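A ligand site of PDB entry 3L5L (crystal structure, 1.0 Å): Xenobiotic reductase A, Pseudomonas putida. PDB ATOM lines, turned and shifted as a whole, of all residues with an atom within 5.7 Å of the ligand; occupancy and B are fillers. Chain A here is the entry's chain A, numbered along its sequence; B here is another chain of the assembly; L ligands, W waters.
Water W5 bridges an oxygen (O8) of the ligand (2.7 Å) and the guanidinium group (NH2) of Arg 326 (3.4 Å).
Water W1 lies within hydrogen-bond range of an oxygen (O9) of the ligand (2.8 Å), the backbone NH (N) of Ala 327 (2.8 Å) and the backbone NH (N) of Arg 326 (3.4 Å).
The backbone NH of Arg 326 sits at hydrogen-bond distance from an oxygen (O7) of the ligand, at 2.8 Å.
An oxygen (O7) of the ligand is in salt-bridge range of the guanidinium group (NE) of Arg 326.
OE1 of Gln 99 sits at hydrogen-bond distance from N2 of the ligand (2.8 Å).
An oxygen (O9) of the ligand lies within hydrogen-bond range of the backbone NH (N) of Gly 325.
NH1 of Arg 231 sits at hydrogen-bond distance from O4 of the ligand.
The backbone carbonyl oxygen (O) of Pro 23 is in hydrogen-bond range of an oxygen (O3) of the ligand, at 2.9 Å.
N3 of the ligand sits at hydrogen-bond distance from N of Cys 25 (2.9 Å).
An oxygen (O2) of the ligand is in hydrogen-bond range of the side-chain sulfur (SG) of Cys 25 (3.3 Å).
The backbone NH (N) of Gly 303 is in hydrogen-bond range of an oxygen (O8) of the ligand, 2.9 Å away.
N of Ala 57 sits at hydrogen-bond distance from O2 of the ligand (3.0 Å).
The backbone NH (N) of Trp 302 lies within hydrogen-bond range of an oxygen (O6) of the ligand (3.4 Å).
O1 of the ligand lies within hydrogen-bond range of NE2 of His 178, 3.3 Å away.
Merely in contact with the ligand: Pro 22 (3.4 Å), Met 24 (3.4 Å), Glu 56 (3.9 Å), His 181 (3.4 Å), Ala 301 (3.4 Å), Val 324 (3.8 Å), Leu 329 (3.99 Å) and Trp 358 of chain B (3.2 Å).
Hydrophobic or aromatic side chains within 4 Å of the ligand: Pro 22, Pro 23, Met 24, Ala 57, His 178, His 181, Ala 301, Trp 302, Leu 329 and Trp 358 of chain B.
The nearest printed residue that does not touch the ligand is Ser 323 (4.3 Å).
The side-chain amide oxygen (OE1) of Gln 99 sits close to the backbone NH (N) of Ala 57 (3.4 Å).
The side-chain amide nitrogen of Gln 99 sits at hydrogen-bond distance from the side-chain carboxylate of Glu 176 (2.7 Å).
The backbone NH of Ala 180 sits at hydrogen-bond distance from the backbone carbonyl oxygen of Arg 231, at 3.3 Å.
The indole nitrogen (NE1) of Trp 358 of chain B lies close to the backbone carbonyl oxygen (O) of Pro 354 of chain B (3.4 Å).
A ring nitrogen (ND1) of His 178 lies within hydrogen-bond range of the backbone NH (N) of Ala 180, 3.3 Å away.
The backbone carbonyl oxygen (O) of Met 24 lies within hydrogen-bond range of the side-chain amide nitrogen (NE2) of Gln 26, 3.0 Å away.
NE2 of His 181 lies within hydrogen-bond range of OG of Ser 266, at 2.7 Å.
The side-chain carboxylate (OE1) of Glu 56 lies within hydrogen-bond range of the backbone NH (N) of Gln 26 (3.0 Å).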
ATOM      1  N   PRO A  22     -18.213  13.645  -1.577  1.00  0.00           N
ATOM      2  CA  PRO A  22     -19.302  14.363  -0.931  1.00  0.00           C
ATOM      3  C   PRO A  22     -20.096  13.385  -0.082  1.00  0.00           C
ATOM      4  O   PRO A  22     -20.034  12.165  -0.256  1.00  0.00           O
ATOM      5  CB  PRO A  22     -20.119  14.882  -2.113  1.00  0.00           C
ATOM      6  CG  PRO A  22     -19.942  13.814  -3.150  1.00  0.00           C
ATOM      7  CD  PRO A  22     -18.532  13.362  -2.992  1.00  0.00           C
ATOM      8  N   PRO A  23     -20.920  13.940   0.824  1.00  0.00           N
ATOM      9  CA  PRO A  23     -21.773  13.067   1.647  1.00  0.00           C
ATOM     10  C   PRO A  23     -22.694  12.225   0.766  1.00  0.00           C
ATOM     11  O   PRO A  23     -23.347  12.734  -0.145  1.00  0.00           O
ATOM     12  CB  PRO A  23     -22.575  14.069   2.498  1.00  0.00           C
ATOM     13  CG  PRO A  23     -22.511  15.377   1.699  1.00  0.00           C
ATOM     14  CD  PRO A  23     -21.160  15.358   1.084  1.00  0.00           C
ATOM     15  N   MET A  24     -22.739  10.926   1.081  1.00  0.00           N
ATOM     16  CA  MET A  24     -23.629   9.999   0.390  1.00  0.00           C
ATOM     17  C   MET A  24     -24.260   9.022   1.369  1.00  0.00           C
ATOM     18  O   MET A  24     -23.620   8.039   1.803  1.00  0.00           O
ATOM     19  CB  MET A  24     -22.889   9.219  -0.701  1.00  0.00           C
ATOM     20  CG  MET A  24     -22.523  10.073  -1.898  1.00  0.00           C
ATOM     21  SD  MET A  24     -21.683   9.134  -3.224  1.00  0.00           S
ATOM     22  CE  MET A  24     -20.085   8.933  -2.455  1.00  0.00           C
ATOM     23  N   CYS A  25     -25.509   9.276   1.684  1.00  0.00           N
ATOM     24  CA  CYS A  25     -26.319   8.389   2.518  1.00  0.00           C
ATOM     25  C   CYS A  25     -26.209   6.937   2.052  1.00  0.00           C
ATOM     26  O   CYS A  25     -26.315   6.623   0.846  1.00  0.00           O
ATOM     27  CB  CYS A  25     -27.783   8.801   2.473  1.00  0.00           C
ATOM     28  SG  CYS A  25     -28.188  10.233   3.468  1.00  0.00           S
ATOM     29  N   GLN A  26     -26.052   6.058   3.028  1.00  0.00           N
ATOM     30  CA  GLN A  26     -25.937   4.627   2.820  1.00  0.00           C
ATOM     31  C   GLN A  26     -27.195   3.860   3.245  1.00  0.00           C
ATOM     32  O   GLN A  26     -27.382   2.710   2.836  1.00  0.00           O
ATOM     33  CB  GLN A  26     -24.724   4.091   3.583  1.00  0.00           C
ATOM     34  CG  GLN A  26     -23.409   4.696   3.083  1.00  0.00           C
ATOM     35  CD  GLN A  26     -23.151   4.283   1.664  1.00  0.00           C
ATOM     36  OE1 GLN A  26     -22.789   3.140   1.396  1.00  0.00           O
ATOM     37  NE2 GLN A  26     -23.264   5.236   0.734  1.00  0.00           N
ATOM     38  N   TYR A  27     -28.026   4.474   4.099  1.00  0.00           N
ATOM     39  CA  TYR A  27     -29.297   3.878   4.532  1.00  0.00           C
ATOM     40  C   TYR A  27     -29.091   2.536   5.238  1.00  0.00           C
ATOM     41  O   TYR A  27     -29.956   1.676   5.190  1.00  0.00           O
ATOM     42  CB  TYR A  27     -30.287   3.740   3.362  1.00  0.00           C
ATOM     43  CG  TYR A  27     -30.451   5.014   2.554  1.00  0.00           C
ATOM     44  CD1 TYR A  27     -31.350   5.978   2.937  1.00  0.00           C
ATOM     45  CD2 TYR A  27     -29.667   5.248   1.436  1.00  0.00           C
ATOM     46  CE1 TYR A  27     -31.503   7.161   2.196  1.00  0.00           C
ATOM     47  CE2 TYR A  27     -29.795   6.402   0.712  1.00  0.00           C
ATOM     48  CZ  TYR A  27     -30.711   7.355   1.082  1.00  0.00           C
ATOM     49  OH  TYR A  27     -30.826   8.506   0.327  1.00  0.00           O
ATOM     50  N   GLU A  56     -21.842  10.937   5.120  1.00  0.00           N
ATOM     51  CA  GLU A  56     -23.230  11.132   4.788  1.00  0.00           C
ATOM     52  C   GLU A  56     -23.995  11.983   5.788  1.00  0.00           C
ATOM     53  O   GLU A  56     -23.685  12.031   6.980  1.00  0.00           O
ATOM     54  CB  GLU A  56     -23.903   9.754   4.732  1.00  0.00           C
ATOM     55  CG  GLU A  56     -23.943   9.008   6.055  1.00  0.00           C
ATOM     56  CD  GLU A  56     -24.267   7.534   5.818  1.00  0.00           C
ATOM     57  OE1 GLU A  56     -25.481   7.186   5.738  1.00  0.00           O
ATOM     58  OE2 GLU A  56     -23.318   6.735   5.690  1.00  0.00           O
ATOM     59  N   ALA A  57     -25.095  12.562   5.292  1.00  0.00           N
ATOM     60  CA  ALA A  57     -26.041  13.300   6.132  1.00  0.00           C
ATOM     61  C   ALA A  57     -26.334  12.508   7.414  1.00  0.00           C
ATOM     62  O   ALA A  57     -26.931  11.423   7.371  1.00  0.00           O
ATOM     63  CB  ALA A  57     -27.345  13.507   5.379  1.00  0.00           C
ATOM     64  N   GLN A  99     -21.288  15.633   7.391  1.00  0.00           N
ATOM     65  CA  GLN A  99     -22.413  16.509   7.138  1.00  0.00           C
ATOM     66  C   GLN A  99     -23.464  16.249   8.208  1.00  0.00           C
ATOM     67  O   GLN A  99     -23.927  15.130   8.349  1.00  0.00           O
ATOM     68  CB  GLN A  99     -22.996  16.212   5.737  1.00  0.00           C
ATOM     69  CG  GLN A  99     -24.119  17.180   5.367  1.00  0.00           C
ATOM     70  CD  GLN A  99     -24.815  16.777   4.095  1.00  0.00           C
ATOM     71  OE1 GLN A  99     -25.379  15.693   4.024  1.00  0.00           O
ATOM     72  NE2 GLN A  99     -24.805  17.655   3.077  1.00  0.00           N
ATOM     73  N   GLU A 176     -19.846  20.057   7.721  1.00  0.00           N
ATOM     74  CA  GLU A 176     -20.728  20.629   6.707  1.00  0.00           C
ATOM     75  C   GLU A 176     -22.154  20.648   7.226  1.00  0.00           C
ATOM     76  O   GLU A 176     -22.729  19.616   7.529  1.00  0.00           O
ATOM     77  CB  GLU A 176     -20.645  19.788   5.420  1.00  0.00           C
ATOM     78  CG  GLU A 176     -21.431  20.405   4.246  1.00  0.00           C
ATOM     79  CD  GLU A 176     -21.414  19.510   3.018  1.00  0.00           C
ATOM     80  OE1 GLU A 176     -20.338  19.381   2.411  1.00  0.00           O
ATOM     81  OE2 GLU A 176     -22.420  18.939   2.666  1.00  0.00           O
ATOM     82  N   HIS A 178     -25.994  20.834   6.555  1.00  0.00           N
ATOM     83  CA  HIS A 178     -26.814  20.488   5.418  1.00  0.00           C
ATOM     84  C   HIS A 178     -28.001  21.426   5.274  1.00  0.00           C
ATOM     85  O   HIS A 178     -29.091  21.185   5.786  1.00  0.00           O
ATOM     86  CB  HIS A 178     -27.296  19.064   5.506  1.00  0.00           C
ATOM     87  CG  HIS A 178     -27.814  18.534   4.221  1.00  0.00           C
ATOM     88  ND1 HIS A 178     -27.984  19.330   3.099  1.00  0.00           N
ATOM     89  CD2 HIS A 178     -28.104  17.265   3.848  1.00  0.00           C
ATOM     90  CE1 HIS A 178     -28.365  18.545   2.103  1.00  0.00           C
ATOM     91  NE2 HIS A 178     -28.416  17.290   2.516  1.00  0.00           N
ATOM     92  N   ALA A 180     -29.189  22.240   2.233  1.00  0.00           N
ATOM     93  CA  ALA A 180     -29.568  22.057   0.832  1.00  0.00           C
ATOM     94  C   ALA A 180     -30.665  21.010   0.689  1.00  0.00           C
ATOM     95  O   ALA A 180     -31.156  20.424   1.661  1.00  0.00           O
ATOM     96  CB  ALA A 180     -28.336  21.688  -0.011  1.00  0.00           C
ATOM     97  N   HIS A 181     -31.088  20.823  -0.553  1.00  0.00           N
ATOM     98  CA  HIS A 181     -31.831  19.658  -0.992  1.00  0.00           C
ATOM     99  C   HIS A 181     -33.238  19.545  -0.392  1.00  0.00           C
ATOM    100  O   HIS A 181     -33.803  18.460  -0.332  1.00  0.00           O
ATOM    101  CB  HIS A 181     -31.019  18.369  -0.815  1.00  0.00           C
ATOM    102  CG  HIS A 181     -29.706  18.392  -1.547  1.00  0.00           C
ATOM    103  ND1 HIS A 181     -28.714  17.470  -1.308  1.00  0.00           N
ATOM    104  CD2 HIS A 181     -29.222  19.224  -2.518  1.00  0.00           C
ATOM    105  CE1 HIS A 181     -27.678  17.733  -2.084  1.00  0.00           C
ATOM    106  NE2 HIS A 181     -27.957  18.777  -2.834  1.00  0.00           N
ATOM    107  N   ARG A 231     -23.590  23.128   2.883  1.00  0.00           N
ATOM    108  CA  ARG A 231     -24.152  22.843   1.567  1.00  0.00           C
ATOM    109  C   ARG A 231     -25.435  23.620   1.472  1.00  0.00           C
ATOM    110  O   ARG A 231     -26.249  23.625   2.406  1.00  0.00           O
ATOM    111  CB  ARG A 231     -24.372  21.342   1.371  1.00  0.00           C
ATOM    112  CG  ARG A 231     -24.516  20.983  -0.119  1.00  0.00           C
ATOM    113  CD  ARG A 231     -24.417  19.495  -0.378  1.00  0.00           C
ATOM    114  NE  ARG A 231     -23.913  19.267  -1.732  1.00  0.00           N
ATOM    115  CZ  ARG A 231     -23.705  18.083  -2.269  1.00  0.00           C
ATOM    116  NH1 ARG A 231     -23.078  17.987  -3.452  1.00  0.00           N
ATOM    117  NH2 ARG A 231     -24.078  16.981  -1.663  1.00  0.00           N
ATOM    118  N   SER A 266     -25.222  23.740  -4.429  1.00  0.00           N
ATOM    119  CA  SER A 266     -26.090  22.743  -4.978  1.00  0.00           C
ATOM    120  C   SER A 266     -27.380  23.355  -5.468  1.00  0.00           C
ATOM    121  O   SER A 266     -27.520  24.575  -5.592  1.00  0.00           O
ATOM    122  CB  SER A 266     -26.301  21.627  -3.950  1.00  0.00           C
ATOM    123  OG  SER A 266     -26.824  20.465  -4.581  1.00  0.00           O
ATOM    124  N   ALA A 301     -20.863  19.415  -7.432  1.00  0.00           N
ATOM    125  CA  ALA A 301     -20.925  18.029  -7.824  1.00  0.00           C
ATOM    126  C   ALA A 301     -21.867  17.913  -8.999  1.00  0.00           C
ATOM    127  O   ALA A 301     -22.582  18.862  -9.320  1.00  0.00           O
ATOM    128  CB  ALA A 301     -21.439  17.160  -6.658  1.00  0.00           C
ATOM    129  N   TRP A 302     -21.847  16.720  -9.587  1.00  0.00           N
ATOM    130  CA  TRP A 302     -22.749  16.160 -10.592  1.00  0.00           C
ATOM    131  C   TRP A 302     -21.953  15.969 -11.874  1.00  0.00           C
ATOM    132  O   TRP A 302     -21.759  16.909 -12.659  1.00  0.00           O
ATOM    133  CB  TRP A 302     -24.036  16.923 -10.863  1.00  0.00           C
ATOM    134  CG  TRP A 302     -24.927  16.091 -11.761  1.00  0.00           C
ATOM    135  CD1 TRP A 302     -24.890  15.970 -13.151  1.00  0.00           C
ATOM    136  CD2 TRP A 302     -25.987  15.250 -11.339  1.00  0.00           C
ATOM    137  NE1 TRP A 302     -25.867  15.117 -13.580  1.00  0.00           N
ATOM    138  CE2 TRP A 302     -26.541  14.640 -12.487  1.00  0.00           C
ATOM    139  CE3 TRP A 302     -26.513  14.942 -10.077  1.00  0.00           C
ATOM    140  CZ2 TRP A 302     -27.624  13.747 -12.410  1.00  0.00           C
ATOM    141  CZ3 TRP A 302     -27.557  14.056  -9.997  1.00  0.00           C
ATOM    142  CH2 TRP A 302     -28.115  13.466 -11.152  1.00  0.00           C
ATOM    143  N   GLY A 303     -21.491  14.751 -12.068  1.00  0.00           N
ATOM    144  CA  GLY A 303     -20.817  14.372 -13.297  1.00  0.00           C
ATOM    145  C   GLY A 303     -19.304  14.604 -13.343  1.00  0.00           C
ATOM    146  O   GLY A 303     -18.705  14.494 -14.408  1.00  0.00           O
ATOM    147  N   PHE A 304     -18.661  14.917 -12.221  1.00  0.00           N
ATOM    148  CA  PHE A 304     -17.210  15.127 -12.212  1.00  0.00           C
ATOM    149  C   PHE A 304     -16.342  13.857 -12.141  1.00  0.00           C
ATOM    150  O   PHE A 304     -15.118  13.936 -12.055  1.00  0.00           O
ATOM    151  CB  PHE A 304     -16.813  16.108 -11.121  1.00  0.00           C
ATOM    152  CG  PHE A 304     -17.252  17.518 -11.391  1.00  0.00           C
ATOM    153  CD1 PHE A 304     -16.556  18.293 -12.320  1.00  0.00           C
ATOM    154  CD2 PHE A 304     -18.353  18.077 -10.732  1.00  0.00           C
ATOM    155  CE1 PHE A 304     -16.925  19.589 -12.555  1.00  0.00           C
ATOM    156  CE2 PHE A 304     -18.741  19.369 -10.968  1.00  0.00           C
ATOM    157  CZ  PHE A 304     -18.026  20.146 -11.886  1.00  0.00           C
ATOM    158  N   GLY A 305     -16.995  12.703 -12.218  1.00  0.00           N
ATOM    159  CA  GLY A 305     -16.257  11.445 -12.324  1.00  0.00           C
ATOM    160  C   GLY A 305     -15.481  11.263 -13.626  1.00  0.00           C
ATOM    161  O   GLY A 305     -14.693  10.337 -13.744  1.00  0.00           O
ATOM    162  N   SER A 323     -16.161  17.659  -6.050  1.00  0.00           N
ATOM    163  CA  SER A 323     -16.850  16.573  -5.366  1.00  0.00           C
ATOM    164  C   SER A 323     -17.244  15.489  -6.383  1.00  0.00           C
ATOM    165  O   SER A 323     -17.901  15.784  -7.382  1.00  0.00           O
ATOM    166  CB  SER A 323     -18.072  17.097  -4.638  1.00  0.00           C
ATOM    167  OG  SER A 323     -17.672  17.968  -3.575  1.00  0.00           O
ATOM    168  N   VAL A 324     -16.862  14.257  -6.076  1.00  0.00           N
ATOM    169  CA  VAL A 324     -17.050  13.098  -6.943  1.00  0.00           C
ATOM    170  C   VAL A 324     -17.767  12.007  -6.140  1.00  0.00           C
ATOM    171  O   VAL A 324     -17.157  11.408  -5.236  1.00  0.00           O
ATOM    172  CB  VAL A 324     -15.726  12.608  -7.498  1.00  0.00           C
ATOM    173  CG1 VAL A 324     -15.950  11.383  -8.388  1.00  0.00           C
ATOM    174  CG2 VAL A 324     -15.004  13.715  -8.268  1.00  0.00           C
ATOM    175  N   GLY A 325     -19.044  11.802  -6.413  1.00  0.00           N
ATOM    176  CA  GLY A 325     -19.902  10.924  -5.631  1.00  0.00           C
ATOM    177  C   GLY A 325     -20.041   9.544  -6.219  1.00  0.00           C
ATOM    178  O   GLY A 325     -19.354   8.594  -5.797  1.00  0.00           O
ATOM    179  N   ARG A 326     -20.974   9.379  -7.147  1.00  0.00           N
ATOM    180  CA  ARG A 326     -21.312   8.049  -7.655  1.00  0.00           C
ATOM    181  C   ARG A 326     -20.129   7.285  -8.223  1.00  0.00           C
ATOM    182  O   ARG A 326     -20.048   6.055  -8.114  1.00  0.00           O
ATOM    183  CB  ARG A 326     -22.456   8.110  -8.648  1.00  0.00           C
ATOM    184  CG  ARG A 326     -23.804   8.297  -7.974  1.00  0.00           C
ATOM    185  CD  ARG A 326     -24.903   8.688  -8.908  1.00  0.00           C
ATOM    186  NE  ARG A 326     -24.677  10.034  -9.418  1.00  0.00           N
ATOM    187  CZ  ARG A 326     -25.467  10.605 -10.306  1.00  0.00           C
ATOM    188  NH1 ARG A 326     -26.558   9.976 -10.733  1.00  0.00           N
ATOM    189  NH2 ARG A 326     -25.157  11.804 -10.756  1.00  0.00           N
ATOM    190  N   ALA A 327     -19.167   7.972  -8.839  1.00  0.00           N
ATOM    191  CA  ALA A 327     -17.989   7.273  -9.366  1.00  0.00           C
ATOM    192  C   ALA A 327     -17.219   6.552  -8.271  1.00  0.00           C
ATOM    193  O   ALA A 327     -16.556   5.555  -8.559  1.00  0.00           O
ATOM    194  CB  ALA A 327     -17.085   8.231 -10.141  1.00  0.00           C
ATOM    195  N   LEU A 329     -18.763   5.169  -5.589  1.00  0.00           N
ATOM    196  CA  LEU A 329     -19.529   3.964  -5.295  1.00  0.00           C
ATOM    197  C   LEU A 329     -19.165   2.867  -6.306  1.00  0.00           C
ATOM    198  O   LEU A 329     -18.993   1.700  -5.958  1.00  0.00           O
ATOM    199  CB  LEU A 329     -21.029   4.244  -5.334  1.00  0.00           C
ATOM    200  CG  LEU A 329     -21.534   5.398  -4.472  1.00  0.00           C
ATOM    201  CD1 LEU A 329     -23.025   5.542  -4.554  1.00  0.00           C
ATOM    202  CD2 LEU A 329     -21.105   5.240  -3.005  1.00  0.00           C
ATOM    203  N   PRO B 354     -26.786  -0.306  -1.375  1.00  0.00           N
ATOM    204  CA  PRO B 354     -26.404   1.109  -1.216  1.00  0.00           C
ATOM    205  C   PRO B 354     -25.497   1.654  -2.306  1.00  0.00           C
ATOM    206  O   PRO B 354     -25.331   2.859  -2.397  1.00  0.00           O
ATOM    207  CB  PRO B 354     -25.708   1.145   0.156  1.00  0.00           C
ATOM    208  CG  PRO B 354     -26.221  -0.078   0.886  1.00  0.00           C
ATOM    209  CD  PRO B 354     -26.435  -1.118  -0.185  1.00  0.00           C
ATOM    210  N   TRP B 358     -27.916   3.160  -7.231  1.00  0.00           N
ATOM    211  CA  TRP B 358     -27.549   4.443  -7.816  1.00  0.00           C
ATOM    212  C   TRP B 358     -26.780   4.302  -9.121  1.00  0.00           C
ATOM    213  O   TRP B 358     -26.560   5.274  -9.818  1.00  0.00           O
ATOM    214  CB  TRP B 358     -26.689   5.234  -6.825  1.00  0.00           C
ATOM    215  CG  TRP B 358     -27.322   5.310  -5.524  1.00  0.00           C
ATOM    216  CD1 TRP B 358     -27.017   4.566  -4.426  1.00  0.00           C
ATOM    217  CD2 TRP B 358     -28.481   6.056  -5.202  1.00  0.00           C
ATOM    218  NE1 TRP B 358     -27.909   4.844  -3.419  1.00  0.00           N
ATOM    219  CE2 TRP B 358     -28.805   5.776  -3.864  1.00  0.00           C
ATOM    220  CE3 TRP B 358     -29.262   6.981  -5.906  1.00  0.00           C
ATOM    221  CZ2 TRP B 358     -29.877   6.354  -3.221  1.00  0.00           C
ATOM    222  CZ3 TRP B 358     -30.332   7.550  -5.265  1.00  0.00           C
ATOM    223  CH2 TRP B 358     -30.628   7.235  -3.932  1.00  0.00           C
HETATM  224  N1  LIG L   1     -26.022  14.865  -0.843  1.00  0.00           N
HETATM  225  C1  LIG L   1     -25.960  15.441   0.406  1.00  0.00           C
HETATM  226  O1  LIG L   1     -25.814  16.642   0.578  1.00  0.00           O
HETATM  227  N2  LIG L   1     -25.993  14.584   1.528  1.00  0.00           N
HETATM  228  C2  LIG L   1     -26.165  13.207   1.457  1.00  0.00           C
HETATM  229  O2  LIG L   1     -26.059  12.529   2.475  1.00  0.00           O
HETATM  230  C3  LIG L   1     -26.409  12.709   0.131  1.00  0.00           C
HETATM  231  N3  LIG L   1     -26.684  11.362  -0.001  1.00  0.00           N
HETATM  232  C4  LIG L   1     -26.502  10.811  -1.294  1.00  0.00           C
HETATM  233  C5  LIG L   1     -26.536   9.415  -1.392  1.00  0.00           C
HETATM  234  C6  LIG L   1     -26.206   8.810  -2.615  1.00  0.00           C
HETATM  235  C7  LIG L   1     -26.062   7.321  -2.679  1.00  0.00           C
HETATM  236  C8  LIG L   1     -25.965   9.636  -3.722  1.00  0.00           C
HETATM  237  C9  LIG L   1     -25.640   9.012  -5.091  1.00  0.00           C
HETATM  238  C10 LIG L   1     -25.965  10.993  -3.623  1.00  0.00           C
HETATM  239  C11 LIG L   1     -26.206  11.613  -2.381  1.00  0.00           C
HETATM  240  N4  LIG L   1     -26.115  13.001  -2.222  1.00  0.00           N
HETATM  241  C12 LIG L   1     -26.184  13.558  -0.952  1.00  0.00           C
HETATM  242  C13 LIG L   1     -25.641  13.861  -3.381  1.00  0.00           C
HETATM  243  C14 LIG L   1     -24.216  13.673  -3.625  1.00  0.00           C
HETATM  244  O3  LIG L   1     -23.413  14.257  -2.581  1.00  0.00           O
HETATM  245  C15 LIG L   1     -23.722  14.350  -4.968  1.00  0.00           C
HETATM  246  O4  LIG L   1     -23.980  15.748  -4.935  1.00  0.00           O
HETATM  247  C16 LIG L   1     -24.428  13.711  -6.199  1.00  0.00           C
HETATM  248  O5  LIG L   1     -24.371  12.309  -6.141  1.00  0.00           O
HETATM  249  C17 LIG L   1     -23.868  14.242  -7.512  1.00  0.00           C
HETATM  250  O6  LIG L   1     -22.475  13.921  -7.679  1.00  0.00           O
HETATM  251  P1  LIG L   1     -22.047  12.673  -8.631  1.00  0.00           P
HETATM  252  O7  LIG L   1     -22.658  11.429  -8.022  1.00  0.00           O
HETATM  253  O8  LIG L   1     -22.602  12.931 -10.038  1.00  0.00           O
HETATM  254  O9  LIG L   1     -20.597  12.699  -8.563  1.00  0.00           O
HETATM  255  O   HOH W   1     -19.214  10.636  -9.799  1.00  0.00           O
HETATM  256  O   HOH W   2     -27.256  11.729  -7.209  1.00  0.00           O
HETATM  257  O   HOH W   3     -19.565  15.006  -9.408  1.00  0.00           O
HETATM  258  O   HOH W   4     -28.708  15.126  -4.013  1.00  0.00           O
HETATM  259  O   HOH W   5     -22.088  11.155 -12.041  1.00  0.00           O
